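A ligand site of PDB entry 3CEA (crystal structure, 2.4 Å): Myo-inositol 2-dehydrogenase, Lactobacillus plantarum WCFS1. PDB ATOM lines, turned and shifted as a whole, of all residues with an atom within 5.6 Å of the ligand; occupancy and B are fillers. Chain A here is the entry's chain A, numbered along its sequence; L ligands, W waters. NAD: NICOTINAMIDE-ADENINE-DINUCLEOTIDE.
N of Arg 18 is in hydrogen-bond range of O1A of the ligand, 3.0 Å away. An oxygen (O2N) of the ligand is in salt-bridge range of the guanidinium group (NH1) of Arg 18, at 2.5 Å. OE1 of Gln 46 sits at hydrogen-bond distance from O3B of the ligand (2.5 Å). The backbone carbonyl oxygen of Lys 102 is in hydrogen-bond range of an oxygen (O2D) of the ligand (2.7 Å). N7N of the ligand sits at hydrogen-bond distance from OE1 of Glu 101 (2.9 Å). O2B of the ligand is in hydrogen-bond range of N of Leu 42. A ring nitrogen (NE2) of His 84 is in hydrogen-bond range of an oxygen (O3D) of the ligand, at 3.0 Å. N of Leu 19 is in hydrogen-bond range of O1N of the ligand. The backbone carbonyl oxygen of Ala 79 sits at hydrogen-bond distance from an oxygen (O3D) of the ligand (3.0 Å). N of Thr 81 is in hydrogen-bond range of O3D of the ligand (3.2 Å). An oxygen (O3D) of the ligand is in hydrogen-bond range of the side-chain hydroxyl (OG1) of Thr 81 (3.1 Å). N7N of the ligand lies within hydrogen-bond range of SD of Met 131 (3.8 Å). An oxygen (O3B) of the ligand lies within hydrogen-bond range of the backbone NH of Leu 16, 3.2 Å away. O7N of the ligand sits close to NE2 of His 189, 3.3 Å away. O3B of the ligand is in hydrogen-bond range of N of Gly 17 (3.4 Å). The backbone carbonyl oxygen of Gly 129 sits at hydrogen-bond distance from a nitrogen (N7N) of the ligand.
Water W2 lies within hydrogen-bond range of O of Val 78 (2.6 Å), O1N of the ligand (2.7 Å), N of Gly 17 (2.9 Å) and N of Gly 20 (3.2 Å).
Merely in contact with the ligand: Pro 80, Val 78, Phe 173, Gly 15, Met 87, Pro 103, Asp 43, Phe 290, Phe 83, Ala 41, Ile 14, Phe 298, Cys 40 and Gly 20. Hydrophobic or aromatic side chains within 4 Å of the ligand: Ile 14, Leu 19, Ala 41, Leu 42, Val 78, Pro 80, Phe 83, His 84, Met 87, Pro 103, Met 131, Phe 173, His 189, Phe 290 and Phe 298. Of the 33 residues printed, 28 come within 4 Å of the ligand.
OD1 of Asp 43 lies within hydrogen-bond range of N of Gln 46, at 3.3 Å. NZ of Lys 102 is in salt-bridge range of OD1 of Asp 185 (3.9 Å). O of Ala 79 sits at hydrogen-bond distance from NE2 of His 84, at 2.6 Å. A ring nitrogen (ND1) of His 84 lies within hydrogen-bond range of the backbone carbonyl oxygen (O) of Pro 103 (2.7 Å). O of Ile 14 is in hydrogen-bond range of N of Val 78 (2.8 Å). The backbone carbonyl oxygen (O) of Cys 40 lies within hydrogen-bond range of the backbone NH (N) of Gly 15, at 2.7 Å. The side-chain sulfur of Cys 40 lies close to the backbone carbonyl oxygen of Thr 61 (3.8 Å). The backbone NH of Tyr 63 lies within hydrogen-bond range of the side-chain sulfur of Cys 40.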
ATOM      1  N   ILE A  14       6.514  27.618 -20.939  1.00  0.00           N
ATOM      2  CA  ILE A  14       5.576  28.346 -21.791  1.00  0.00           C
ATOM      3  C   ILE A  14       5.234  27.444 -22.977  1.00  0.00           C
ATOM      4  O   ILE A  14       6.115  26.928 -23.650  1.00  0.00           O
ATOM      5  CB  ILE A  14       6.149  29.693 -22.293  1.00  0.00           C
ATOM      6  CG1 ILE A  14       6.716  30.521 -21.130  1.00  0.00           C
ATOM      7  CG2 ILE A  14       5.084  30.477 -23.051  1.00  0.00           C
ATOM      8  CD1 ILE A  14       7.593  31.677 -21.560  1.00  0.00           C
ATOM      9  N   GLY A  15       3.931  27.254 -23.201  1.00  0.00           N
ATOM     10  CA  GLY A  15       3.450  26.429 -24.307  1.00  0.00           C
ATOM     11  C   GLY A  15       3.276  24.972 -23.921  1.00  0.00           C
ATOM     12  O   GLY A  15       4.181  24.355 -23.372  1.00  0.00           O
ATOM     13  N   LEU A  16       2.095  24.445 -24.219  1.00  0.00           N
ATOM     14  CA  LEU A  16       1.772  23.038 -23.924  1.00  0.00           C
ATOM     15  C   LEU A  16       1.133  22.348 -25.125  1.00  0.00           C
ATOM     16  O   LEU A  16       0.290  21.454 -24.973  1.00  0.00           O
ATOM     17  CB  LEU A  16       0.854  22.949 -22.694  1.00  0.00           C
ATOM     18  CG  LEU A  16       1.368  23.468 -21.342  1.00  0.00           C
ATOM     19  CD1 LEU A  16       0.227  23.502 -20.330  1.00  0.00           C
ATOM     20  CD2 LEU A  16       2.533  22.633 -20.810  1.00  0.00           C
ATOM     21  N   GLY A  17       1.554  22.750 -26.328  1.00  0.00           N
ATOM     22  CA  GLY A  17       1.011  22.199 -27.567  1.00  0.00           C
ATOM     23  C   GLY A  17       1.613  20.861 -27.963  1.00  0.00           C
ATOM     24  O   GLY A  17       1.870  20.021 -27.107  1.00  0.00           O
ATOM     25  N   ARG A  18       1.855  20.692 -29.264  1.00  0.00           N
ATOM     26  CA  ARG A  18       2.374  19.447 -29.822  1.00  0.00           C
ATOM     27  C   ARG A  18       3.659  18.964 -29.141  1.00  0.00           C
ATOM     28  O   ARG A  18       3.817  17.770 -28.867  1.00  0.00           O
ATOM     29  CB  ARG A  18       2.602  19.599 -31.332  1.00  0.00           C
ATOM     30  CG  ARG A  18       1.316  19.645 -32.145  1.00  0.00           C
ATOM     31  CD  ARG A  18       1.478  20.424 -33.452  1.00  0.00           C
ATOM     32  NE  ARG A  18       2.510  19.870 -34.335  1.00  0.00           N
ATOM     33  CZ  ARG A  18       3.505  20.573 -34.873  1.00  0.00           C
ATOM     34  NH1 ARG A  18       3.615  21.878 -34.638  1.00  0.00           N
ATOM     35  NH2 ARG A  18       4.383  19.975 -35.660  1.00  0.00           N
ATOM     36  N   LEU A  19       4.569  19.905 -28.876  1.00  0.00           N
ATOM     37  CA  LEU A  19       5.823  19.569 -28.214  1.00  0.00           C
ATOM     38  C   LEU A  19       5.797  19.912 -26.736  1.00  0.00           C
ATOM     39  O   LEU A  19       6.374  19.190 -25.914  1.00  0.00           O
ATOM     40  CB  LEU A  19       7.008  20.250 -28.913  1.00  0.00           C
ATOM     41  CG  LEU A  19       8.424  19.943 -28.408  1.00  0.00           C
ATOM     42  CD1 LEU A  19       8.700  18.433 -28.338  1.00  0.00           C
ATOM     43  CD2 LEU A  19       9.437  20.624 -29.273  1.00  0.00           C
ATOM     44  N   GLY A  20       5.119  21.012 -26.395  1.00  0.00           N
ATOM     45  CA  GLY A  20       5.008  21.484 -25.020  1.00  0.00           C
ATOM     46  C   GLY A  20       4.525  20.424 -24.048  1.00  0.00           C
ATOM     47  O   GLY A  20       5.104  20.262 -22.971  1.00  0.00           O
ATOM     48  N   CYS A  40       2.455  28.213 -18.631  1.00  0.00           N
ATOM     49  CA  CYS A  40       1.777  29.301 -19.337  1.00  0.00           C
ATOM     50  C   CYS A  40       1.346  28.872 -20.731  1.00  0.00           C
ATOM     51  O   CYS A  40       2.153  28.391 -21.532  1.00  0.00           O
ATOM     52  CB  CYS A  40       2.684  30.532 -19.402  1.00  0.00           C
ATOM     53  SG  CYS A  40       1.899  31.983 -20.144  1.00  0.00           S
ATOM     54  N   ALA A  41       0.056  29.046 -21.013  1.00  0.00           N
ATOM     55  CA  ALA A  41      -0.523  28.779 -22.332  1.00  0.00           C
ATOM     56  C   ALA A  41      -1.726  29.695 -22.574  1.00  0.00           C
ATOM     57  O   ALA A  41      -2.284  30.260 -21.624  1.00  0.00           O
ATOM     58  CB  ALA A  41      -0.924  27.315 -22.461  1.00  0.00           C
ATOM     59  N   LEU A  42      -2.118  29.849 -23.833  1.00  0.00           N
ATOM     60  CA  LEU A  42      -3.313  30.606 -24.189  1.00  0.00           C
ATOM     61  C   LEU A  42      -4.555  29.703 -24.234  1.00  0.00           C
ATOM     62  O   LEU A  42      -5.688  30.200 -24.313  1.00  0.00           O
ATOM     63  CB  LEU A  42      -3.129  31.340 -25.515  1.00  0.00           C
ATOM     64  CG  LEU A  42      -2.035  32.410 -25.632  1.00  0.00           C
ATOM     65  CD1 LEU A  42      -1.988  32.972 -27.042  1.00  0.00           C
ATOM     66  CD2 LEU A  42      -2.213  33.538 -24.612  1.00  0.00           C
ATOM     67  N   ASP A  43      -4.326  28.396 -24.183  1.00  0.00           N
ATOM     68  CA  ASP A  43      -5.402  27.409 -24.163  1.00  0.00           C
ATOM     69  C   ASP A  43      -5.759  27.042 -22.723  1.00  0.00           C
ATOM     70  O   ASP A  43      -4.895  26.613 -21.949  1.00  0.00           O
ATOM     71  CB  ASP A  43      -4.965  26.150 -24.936  1.00  0.00           C
ATOM     72  CG  ASP A  43      -6.127  25.200 -25.210  1.00  0.00           C
ATOM     73  OD1 ASP A  43      -6.894  24.864 -24.273  1.00  0.00           O
ATOM     74  OD2 ASP A  43      -6.254  24.761 -26.373  1.00  0.00           O
ATOM     75  N   GLN A  46      -5.543  23.120 -21.788  1.00  0.00           N
ATOM     76  CA  GLN A  46      -4.157  22.669 -21.641  1.00  0.00           C
ATOM     77  C   GLN A  46      -3.627  23.001 -20.245  1.00  0.00           C
ATOM     78  O   GLN A  46      -2.878  22.220 -19.655  1.00  0.00           O
ATOM     79  CB  GLN A  46      -3.263  23.282 -22.711  1.00  0.00           C
ATOM     80  CG  GLN A  46      -3.512  22.740 -24.117  1.00  0.00           C
ATOM     81  CD  GLN A  46      -2.691  23.440 -25.170  1.00  0.00           C
ATOM     82  OE1 GLN A  46      -1.828  24.269 -24.873  1.00  0.00           O
ATOM     83  NE2 GLN A  46      -2.937  23.116 -26.439  1.00  0.00           N
ATOM     84  N   THR A  61      -1.854  32.819 -18.262  1.00  0.00           N
ATOM     85  CA  THR A  61      -2.083  33.086 -19.681  1.00  0.00           C
ATOM     86  C   THR A  61      -1.110  34.164 -20.179  1.00  0.00           C
ATOM     87  O   THR A  61      -0.853  34.277 -21.371  1.00  0.00           O
ATOM     88  CB  THR A  61      -3.539  33.544 -19.962  1.00  0.00           C
ATOM     89  OG1 THR A  61      -3.881  34.629 -19.093  1.00  0.00           O
ATOM     90  CG2 THR A  61      -4.514  32.392 -19.747  1.00  0.00           C
ATOM     91  N   TYR A  63       2.753  35.318 -19.913  1.00  0.00           N
ATOM     92  CA  TYR A  63       4.074  34.791 -19.567  1.00  0.00           C
ATOM     93  C   TYR A  63       4.891  35.766 -18.715  1.00  0.00           C
ATOM     94  O   TYR A  63       5.682  35.343 -17.875  1.00  0.00           O
ATOM     95  CB  TYR A  63       4.842  34.343 -20.822  1.00  0.00           C
ATOM     96  CG  TYR A  63       5.441  35.453 -21.660  1.00  0.00           C
ATOM     97  CD1 TYR A  63       4.698  36.061 -22.671  1.00  0.00           C
ATOM     98  CD2 TYR A  63       6.750  35.892 -21.448  1.00  0.00           C
ATOM     99  CE1 TYR A  63       5.242  37.078 -23.452  1.00  0.00           C
ATOM    100  CE2 TYR A  63       7.304  36.917 -22.210  1.00  0.00           C
ATOM    101  CZ  TYR A  63       6.541  37.498 -23.217  1.00  0.00           C
ATOM    102  OH  TYR A  63       7.092  38.510 -23.983  1.00  0.00           O
ATOM    103  N   VAL A  78       8.406  26.751 -25.163  1.00  0.00           N
ATOM    104  CA  VAL A  78       7.853  25.916 -26.228  1.00  0.00           C
ATOM    105  C   VAL A  78       6.605  26.604 -26.812  1.00  0.00           C
ATOM    106  O   VAL A  78       5.619  25.955 -27.150  1.00  0.00           O
ATOM    107  CB  VAL A  78       7.511  24.484 -25.742  1.00  0.00           C
ATOM    108  CG1 VAL A  78       7.532  23.502 -26.900  1.00  0.00           C
ATOM    109  CG2 VAL A  78       8.493  24.028 -24.658  1.00  0.00           C
ATOM    110  N   ALA A  79       6.670  27.934 -26.886  1.00  0.00           N
ATOM    111  CA  ALA A  79       5.658  28.742 -27.553  1.00  0.00           C
ATOM    112  C   ALA A  79       6.066  28.888 -29.022  1.00  0.00           C
ATOM    113  O   ALA A  79       7.188  28.539 -29.373  1.00  0.00           O
ATOM    114  CB  ALA A  79       5.536  30.093 -26.880  1.00  0.00           C
ATOM    115  N   PRO A  80       5.166  29.395 -29.891  1.00  0.00           N
ATOM    116  CA  PRO A  80       5.494  29.585 -31.317  1.00  0.00           C
ATOM    117  C   PRO A  80       6.746  30.431 -31.542  1.00  0.00           C
ATOM    118  O   PRO A  80       7.107  31.258 -30.708  1.00  0.00           O
ATOM    119  CB  PRO A  80       4.259  30.299 -31.869  1.00  0.00           C
ATOM    120  CG  PRO A  80       3.159  29.905 -30.970  1.00  0.00           C
ATOM    121  CD  PRO A  80       3.775  29.792 -29.606  1.00  0.00           C
ATOM    122  N   THR A  81       7.384  30.225 -32.700  1.00  0.00           N
ATOM    123  CA  THR A  81       8.662  30.852 -33.048  1.00  0.00           C
ATOM    124  C   THR A  81       8.724  32.394 -32.959  1.00  0.00           C
ATOM    125  O   THR A  81       9.705  32.933 -32.460  1.00  0.00           O
ATOM    126  CB  THR A  81       9.168  30.367 -34.423  1.00  0.00           C
ATOM    127  OG1 THR A  81       9.168  28.937 -34.452  1.00  0.00           O
ATOM    128  CG2 THR A  81      10.577  30.858 -34.711  1.00  0.00           C
ATOM    129  N   PHE A  83       7.432  34.389 -30.955  1.00  0.00           N
ATOM    130  CA  PHE A  83       7.477  34.833 -29.550  1.00  0.00           C
ATOM    131  C   PHE A  83       8.779  34.479 -28.830  1.00  0.00           C
ATOM    132  O   PHE A  83       9.023  34.928 -27.719  1.00  0.00           O
ATOM    133  CB  PHE A  83       6.281  34.277 -28.775  1.00  0.00           C
ATOM    134  CG  PHE A  83       4.957  34.772 -29.277  1.00  0.00           C
ATOM    135  CD1 PHE A  83       4.470  36.020 -28.896  1.00  0.00           C
ATOM    136  CD2 PHE A  83       4.178  33.981 -30.125  1.00  0.00           C
ATOM    137  CE1 PHE A  83       3.245  36.482 -29.353  1.00  0.00           C
ATOM    138  CE2 PHE A  83       2.941  34.432 -30.587  1.00  0.00           C
ATOM    139  CZ  PHE A  83       2.476  35.689 -30.199  1.00  0.00           C
ATOM    140  N   HIS A  84       9.623  33.681 -29.483  1.00  0.00           N
ATOM    141  CA  HIS A  84      10.889  33.216 -28.906  1.00  0.00           C
ATOM    142  C   HIS A  84      11.853  34.341 -28.484  1.00  0.00           C
ATOM    143  O   HIS A  84      12.334  34.321 -27.354  1.00  0.00           O
ATOM    144  CB  HIS A  84      11.590  32.238 -29.861  1.00  0.00           C
ATOM    145  CG  HIS A  84      10.959  30.893 -29.935  1.00  0.00           C
ATOM    146  ND1 HIS A  84      11.554  29.830 -30.593  1.00  0.00           N
ATOM    147  CD2 HIS A  84       9.800  30.416 -29.431  1.00  0.00           C
ATOM    148  CE1 HIS A  84      10.779  28.768 -30.490  1.00  0.00           C
ATOM    149  NE2 HIS A  84       9.706  29.089 -29.793  1.00  0.00           N
ATOM    150  N   MET A  87      10.407  36.501 -25.516  1.00  0.00           N
ATOM    151  CA  MET A  87      10.294  35.684 -24.302  1.00  0.00           C
ATOM    152  C   MET A  87      11.671  35.408 -23.711  1.00  0.00           C
ATOM    153  O   MET A  87      11.833  35.432 -22.482  1.00  0.00           O
ATOM    154  CB  MET A  87       9.561  34.378 -24.577  1.00  0.00           C
ATOM    155  CG  MET A  87       8.060  34.533 -24.697  1.00  0.00           C
ATOM    156  SD  MET A  87       7.180  32.909 -25.282  1.00  0.00           S
ATOM    157  CE  MET A  87       5.339  33.551 -25.233  1.00  0.00           C
ATOM    158  N   GLU A 101      13.093  26.481 -27.500  1.00  0.00           N
ATOM    159  CA  GLU A 101      12.954  25.582 -28.639  1.00  0.00           C
ATOM    160  C   GLU A 101      13.434  26.226 -29.932  1.00  0.00           C
ATOM    161  O   GLU A 101      13.520  27.456 -30.038  1.00  0.00           O
ATOM    162  CB  GLU A 101      11.510  25.105 -28.794  1.00  0.00           C
ATOM    163  CG  GLU A 101      11.211  23.777 -28.091  1.00  0.00           C
ATOM    164  CD  GLU A 101      12.086  22.614 -28.579  1.00  0.00           C
ATOM    165  OE1 GLU A 101      12.675  22.695 -29.679  1.00  0.00           O
ATOM    166  OE2 GLU A 101      12.171  21.599 -27.852  1.00  0.00           O
ATOM    167  N   LYS A 102      13.763  25.380 -30.900  1.00  0.00           N
ATOM    168  CA  LYS A 102      14.195  25.826 -32.224  1.00  0.00           C
ATOM    169  C   LYS A 102      12.976  26.282 -33.029  1.00  0.00           C
ATOM    170  O   LYS A 102      11.864  25.812 -32.787  1.00  0.00           O
ATOM    171  CB  LYS A 102      14.949  24.691 -32.942  1.00  0.00           C
ATOM    172  CG  LYS A 102      14.084  23.505 -33.361  1.00  0.00           C
ATOM    173  CD  LYS A 102      13.610  23.667 -34.800  1.00  0.00           C
ATOM    174  CE  LYS A 102      12.214  23.108 -34.999  1.00  0.00           C
ATOM    175  NZ  LYS A 102      11.798  23.142 -36.430  1.00  0.00           N
ATOM    176  N   PRO A 103      13.163  27.235 -33.974  1.00  0.00           N
ATOM    177  CA  PRO A 103      14.362  28.029 -34.214  1.00  0.00           C
ATOM    178  C   PRO A 103      14.427  29.208 -33.247  1.00  0.00           C
ATOM    179  O   PRO A 103      13.498  29.415 -32.467  1.00  0.00           O
ATOM    180  CB  PRO A 103      14.180  28.538 -35.652  1.00  0.00           C
ATOM    181  CG  PRO A 103      12.827  28.048 -36.115  1.00  0.00           C
ATOM    182  CD  PRO A 103      12.082  27.564 -34.923  1.00  0.00           C
ATOM    183  N   GLY A 129      17.157  23.965 -29.044  1.00  0.00           N
ATOM    184  CA  GLY A 129      16.494  22.662 -29.109  1.00  0.00           C
ATOM    185  C   GLY A 129      16.801  21.757 -30.288  1.00  0.00           C
ATOM    186  O   GLY A 129      15.896  21.145 -30.859  1.00  0.00           O
ATOM    187  N   MET A 131      17.567  18.621 -30.895  1.00  0.00           N
ATOM    188  CA  MET A 131      17.552  17.356 -30.157  1.00  0.00           C
ATOM    189  C   MET A 131      18.227  16.191 -30.892  1.00  0.00           C
ATOM    190  O   MET A 131      18.716  15.258 -30.247  1.00  0.00           O
ATOM    191  CB  MET A 131      16.119  16.983 -29.730  1.00  0.00           C
ATOM    192  CG  MET A 131      15.258  16.353 -30.830  1.00  0.00           C
ATOM    193  SD  MET A 131      14.830  17.590 -32.270  1.00  0.00           S
ATOM    194  CE  MET A 131      13.861  16.383 -33.393  1.00  0.00           C
ATOM    195  N   PHE A 173      -1.222  24.995 -36.376  1.00  0.00           N
ATOM    196  CA  PHE A 173       0.070  25.524 -35.926  1.00  0.00           C
ATOM    197  C   PHE A 173       0.580  26.660 -36.816  1.00  0.00           C
ATOM    198  O   PHE A 173       1.170  27.616 -36.316  1.00  0.00           O
ATOM    199  CB  PHE A 173       1.081  24.357 -35.872  1.00  0.00           C
ATOM    200  CG  PHE A 173       2.529  24.785 -35.816  1.00  0.00           C
ATOM    201  CD1 PHE A 173       3.099  25.214 -34.620  1.00  0.00           C
ATOM    202  CD2 PHE A 173       3.333  24.702 -36.954  1.00  0.00           C
ATOM    203  CE1 PHE A 173       4.440  25.597 -34.561  1.00  0.00           C
ATOM    204  CE2 PHE A 173       4.675  25.075 -36.912  1.00  0.00           C
ATOM    205  CZ  PHE A 173       5.228  25.522 -35.716  1.00  0.00           C
ATOM    206  N   GLU A 176      -2.198  30.005 -36.998  1.00  0.00           N
ATOM    207  CA  GLU A 176      -2.181  30.813 -35.780  1.00  0.00           C
ATOM    208  C   GLU A 176      -0.903  31.643 -35.632  1.00  0.00           C
ATOM    209  O   GLU A 176      -0.916  32.688 -34.970  1.00  0.00           O
ATOM    210  CB  GLU A 176      -2.407  29.946 -34.537  1.00  0.00           C
ATOM    211  CG  GLU A 176      -3.845  29.469 -34.364  1.00  0.00           C
ATOM    212  CD  GLU A 176      -4.036  28.547 -33.169  1.00  0.00           C
ATOM    213  OE1 GLU A 176      -3.085  27.816 -32.819  1.00  0.00           O
ATOM    214  OE2 GLU A 176      -5.140  28.567 -32.581  1.00  0.00           O
ATOM    215  N   ASP A 185      11.052  25.474 -40.769  1.00  0.00           N
ATOM    216  CA  ASP A 185      10.360  24.597 -39.828  1.00  0.00           C
ATOM    217  C   ASP A 185      10.876  23.162 -39.872  1.00  0.00           C
ATOM    218  O   ASP A 185      11.167  22.570 -38.828  1.00  0.00           O
ATOM    219  CB  ASP A 185       8.845  24.638 -40.043  1.00  0.00           C
ATOM    220  CG  ASP A 185       8.066  24.108 -38.846  1.00  0.00           C
ATOM    221  OD1 ASP A 185       8.380  24.494 -37.696  1.00  0.00           O
ATOM    222  OD2 ASP A 185       7.126  23.314 -39.072  1.00  0.00           O
ATOM    223  N   HIS A 189      16.844  21.304 -38.965  1.00  0.00           N
ATOM    224  CA  HIS A 189      17.462  20.222 -38.204  1.00  0.00           C
ATOM    225  C   HIS A 189      18.588  19.574 -38.983  1.00  0.00           C
ATOM    226  O   HIS A 189      19.676  19.361 -38.444  1.00  0.00           O
ATOM    227  CB  HIS A 189      16.416  19.169 -37.851  1.00  0.00           C
ATOM    228  CG  HIS A 189      15.400  19.627 -36.851  1.00  0.00           C
ATOM    229  ND1 HIS A 189      15.626  19.618 -35.495  1.00  0.00           N
ATOM    230  CD2 HIS A 189      14.141  20.102 -37.024  1.00  0.00           C
ATOM    231  CE1 HIS A 189      14.557  20.068 -34.866  1.00  0.00           C
ATOM    232  NE2 HIS A 189      13.638  20.364 -35.770  1.00  0.00           N
ATOM    233  N   PHE A 290       7.198  12.988 -34.962  1.00  0.00           N
ATOM    234  CA  PHE A 290       8.543  13.384 -34.536  1.00  0.00           C
ATOM    235  C   PHE A 290       8.734  13.105 -33.039  1.00  0.00           C
ATOM    236  O   PHE A 290       9.837  12.760 -32.607  1.00  0.00           O
ATOM    237  CB  PHE A 290       8.785  14.873 -34.847  1.00  0.00           C
ATOM    238  CG  PHE A 290       7.917  15.821 -34.062  1.00  0.00           C
ATOM    239  CD1 PHE A 290       6.625  16.126 -34.495  1.00  0.00           C
ATOM    240  CD2 PHE A 290       8.387  16.407 -32.893  1.00  0.00           C
ATOM    241  CE1 PHE A 290       5.812  17.009 -33.764  1.00  0.00           C
ATOM    242  CE2 PHE A 290       7.583  17.287 -32.160  1.00  0.00           C
ATOM    243  CZ  PHE A 290       6.288  17.579 -32.596  1.00  0.00           C
ATOM    244  N   PHE A 298      14.644  14.047 -26.776  1.00  0.00           N
ATOM    245  CA  PHE A 298      13.985  15.163 -26.093  1.00  0.00           C
ATOM    246  C   PHE A 298      14.212  15.098 -24.586  1.00  0.00           C
ATOM    247  O   PHE A 298      14.430  16.129 -23.949  1.00  0.00           O
ATOM    248  CB  PHE A 298      12.477  15.157 -26.361  1.00  0.00           C
ATOM    249  CG  PHE A 298      12.091  15.714 -27.701  1.00  0.00           C
ATOM    250  CD1 PHE A 298      12.492  17.001 -28.086  1.00  0.00           C
ATOM    251  CD2 PHE A 298      11.298  14.977 -28.570  1.00  0.00           C
ATOM    252  CE1 PHE A 298      12.119  17.519 -29.320  1.00  0.00           C
ATOM    253  CE2 PHE A 298      10.914  15.485 -29.810  1.00  0.00           C
ATOM    254  CZ  PHE A 298      11.330  16.759 -30.186  1.00  0.00           C
ATOM    255  N   GLU A 301      18.153  15.701 -23.865  1.00  0.00           N
ATOM    256  CA  GLU A 301      18.571  17.098 -24.059  1.00  0.00           C
ATOM    257  C   GLU A 301      18.128  18.015 -22.924  1.00  0.00           C
ATOM    258  O   GLU A 301      18.870  18.904 -22.500  1.00  0.00           O
ATOM    259  CB  GLU A 301      18.094  17.661 -25.404  1.00  0.00           C
ATOM    260  CG  GLU A 301      16.603  17.955 -25.492  1.00  0.00           C
ATOM    261  CD  GLU A 301      16.243  18.895 -26.632  1.00  0.00           C
ATOM    262  OE1 GLU A 301      17.160  19.498 -27.239  1.00  0.00           O
ATOM    263  OE2 GLU A 301      15.036  19.027 -26.911  1.00  0.00           O
HETATM  264  PA  NAD L   1       1.677  24.446 -30.857  1.00  0.00           P
HETATM  265  O1A NAD L   1       1.198  23.049 -30.922  1.00  0.00           O
HETATM  266  O2A NAD L   1       0.846  25.360 -31.681  1.00  0.00           O
HETATM  267  O5B NAD L   1       1.718  24.923 -29.320  1.00  0.00           O
HETATM  268  C5B NAD L   1       1.928  26.281 -28.977  1.00  0.00           C
HETATM  269  C4B NAD L   1       1.581  26.513 -27.516  1.00  0.00           C
HETATM  270  O4B NAD L   1       2.052  27.773 -27.074  1.00  0.00           O
HETATM  271  C3B NAD L   1       0.079  26.505 -27.278  1.00  0.00           C
HETATM  272  O3B NAD L   1      -0.177  25.685 -26.158  1.00  0.00           O
HETATM  273  C2B NAD L   1      -0.282  27.942 -26.975  1.00  0.00           C
HETATM  274  O2B NAD L   1      -1.308  28.061 -26.014  1.00  0.00           O
HETATM  275  C1B NAD L   1       1.025  28.526 -26.465  1.00  0.00           C
HETATM  276  N9A NAD L   1       1.152  29.953 -26.809  1.00  0.00           N
HETATM  277  C8A NAD L   1       1.025  30.523 -28.050  1.00  0.00           C
HETATM  278  N7A NAD L   1       1.220  31.866 -27.943  1.00  0.00           N
HETATM  279  C5A NAD L   1       1.470  32.144 -26.646  1.00  0.00           C
HETATM  280  C6A NAD L   1       1.742  33.347 -25.996  1.00  0.00           C
HETATM  281  N6A NAD L   1       2.019  34.434 -26.705  1.00  0.00           N
HETATM  282  N1A NAD L   1       1.965  33.335 -24.627  1.00  0.00           N
HETATM  283  C2A NAD L   1       1.923  32.150 -23.915  1.00  0.00           C
HETATM  284  N3A NAD L   1       1.656  30.964 -24.575  1.00  0.00           N
HETATM  285  C4A NAD L   1       1.437  30.962 -25.924  1.00  0.00           C
HETATM  286  O3  NAD L   1       3.209  24.532 -31.330  1.00  0.00           O
HETATM  287  PN  NAD L   1       4.249  23.323 -31.086  1.00  0.00           P
HETATM  288  O1N NAD L   1       4.031  22.754 -29.732  1.00  0.00           O
HETATM  289  O2N NAD L   1       4.195  22.466 -32.285  1.00  0.00           O
HETATM  290  O5D NAD L   1       5.693  24.030 -31.118  1.00  0.00           O
HETATM  291  C5D NAD L   1       6.002  25.186 -30.381  1.00  0.00           C
HETATM  292  C4D NAD L   1       7.467  25.536 -30.664  1.00  0.00           C
HETATM  293  O4D NAD L   1       8.263  24.362 -30.654  1.00  0.00           O
HETATM  294  C3D NAD L   1       7.636  26.188 -32.034  1.00  0.00           C
HETATM  295  O3D NAD L   1       8.406  27.355 -31.885  1.00  0.00           O
HETATM  296  C2D NAD L   1       8.373  25.153 -32.860  1.00  0.00           C
HETATM  297  O2D NAD L   1       9.328  25.745 -33.706  1.00  0.00           O
HETATM  298  C1D NAD L   1       9.035  24.257 -31.826  1.00  0.00           C
HETATM  299  N1N NAD L   1       9.107  22.854 -32.292  1.00  0.00           N
HETATM  300  C2N NAD L   1      10.322  22.206 -32.249  1.00  0.00           C
HETATM  301  C3N NAD L   1      10.431  20.883 -32.681  1.00  0.00           C
HETATM  302  C7N NAD L   1      11.698  20.111 -32.467  1.00  0.00           C
HETATM  303  O7N NAD L   1      11.933  18.975 -33.283  1.00  0.00           O
HETATM  304  N7N NAD L   1      12.575  20.498 -31.536  1.00  0.00           N
HETATM  305  C4N NAD L   1       9.308  20.226 -33.157  1.00  0.00           C
HETATM  306  C5N NAD L   1       8.077  20.887 -33.208  1.00  0.00           C
HETATM  307  C6N NAD L   1       7.997  22.208 -32.762  1.00  0.00           C
HETATM  308  O   HOH W   1      14.278  20.107 -29.055  1.00  0.00           O
HETATM  309  O   HOH W   2       4.025  23.863 -27.245  1.00  0.00           O
HETATM  310  O   HOH W   3       2.113  37.472 -25.995  1.00  0.00           O
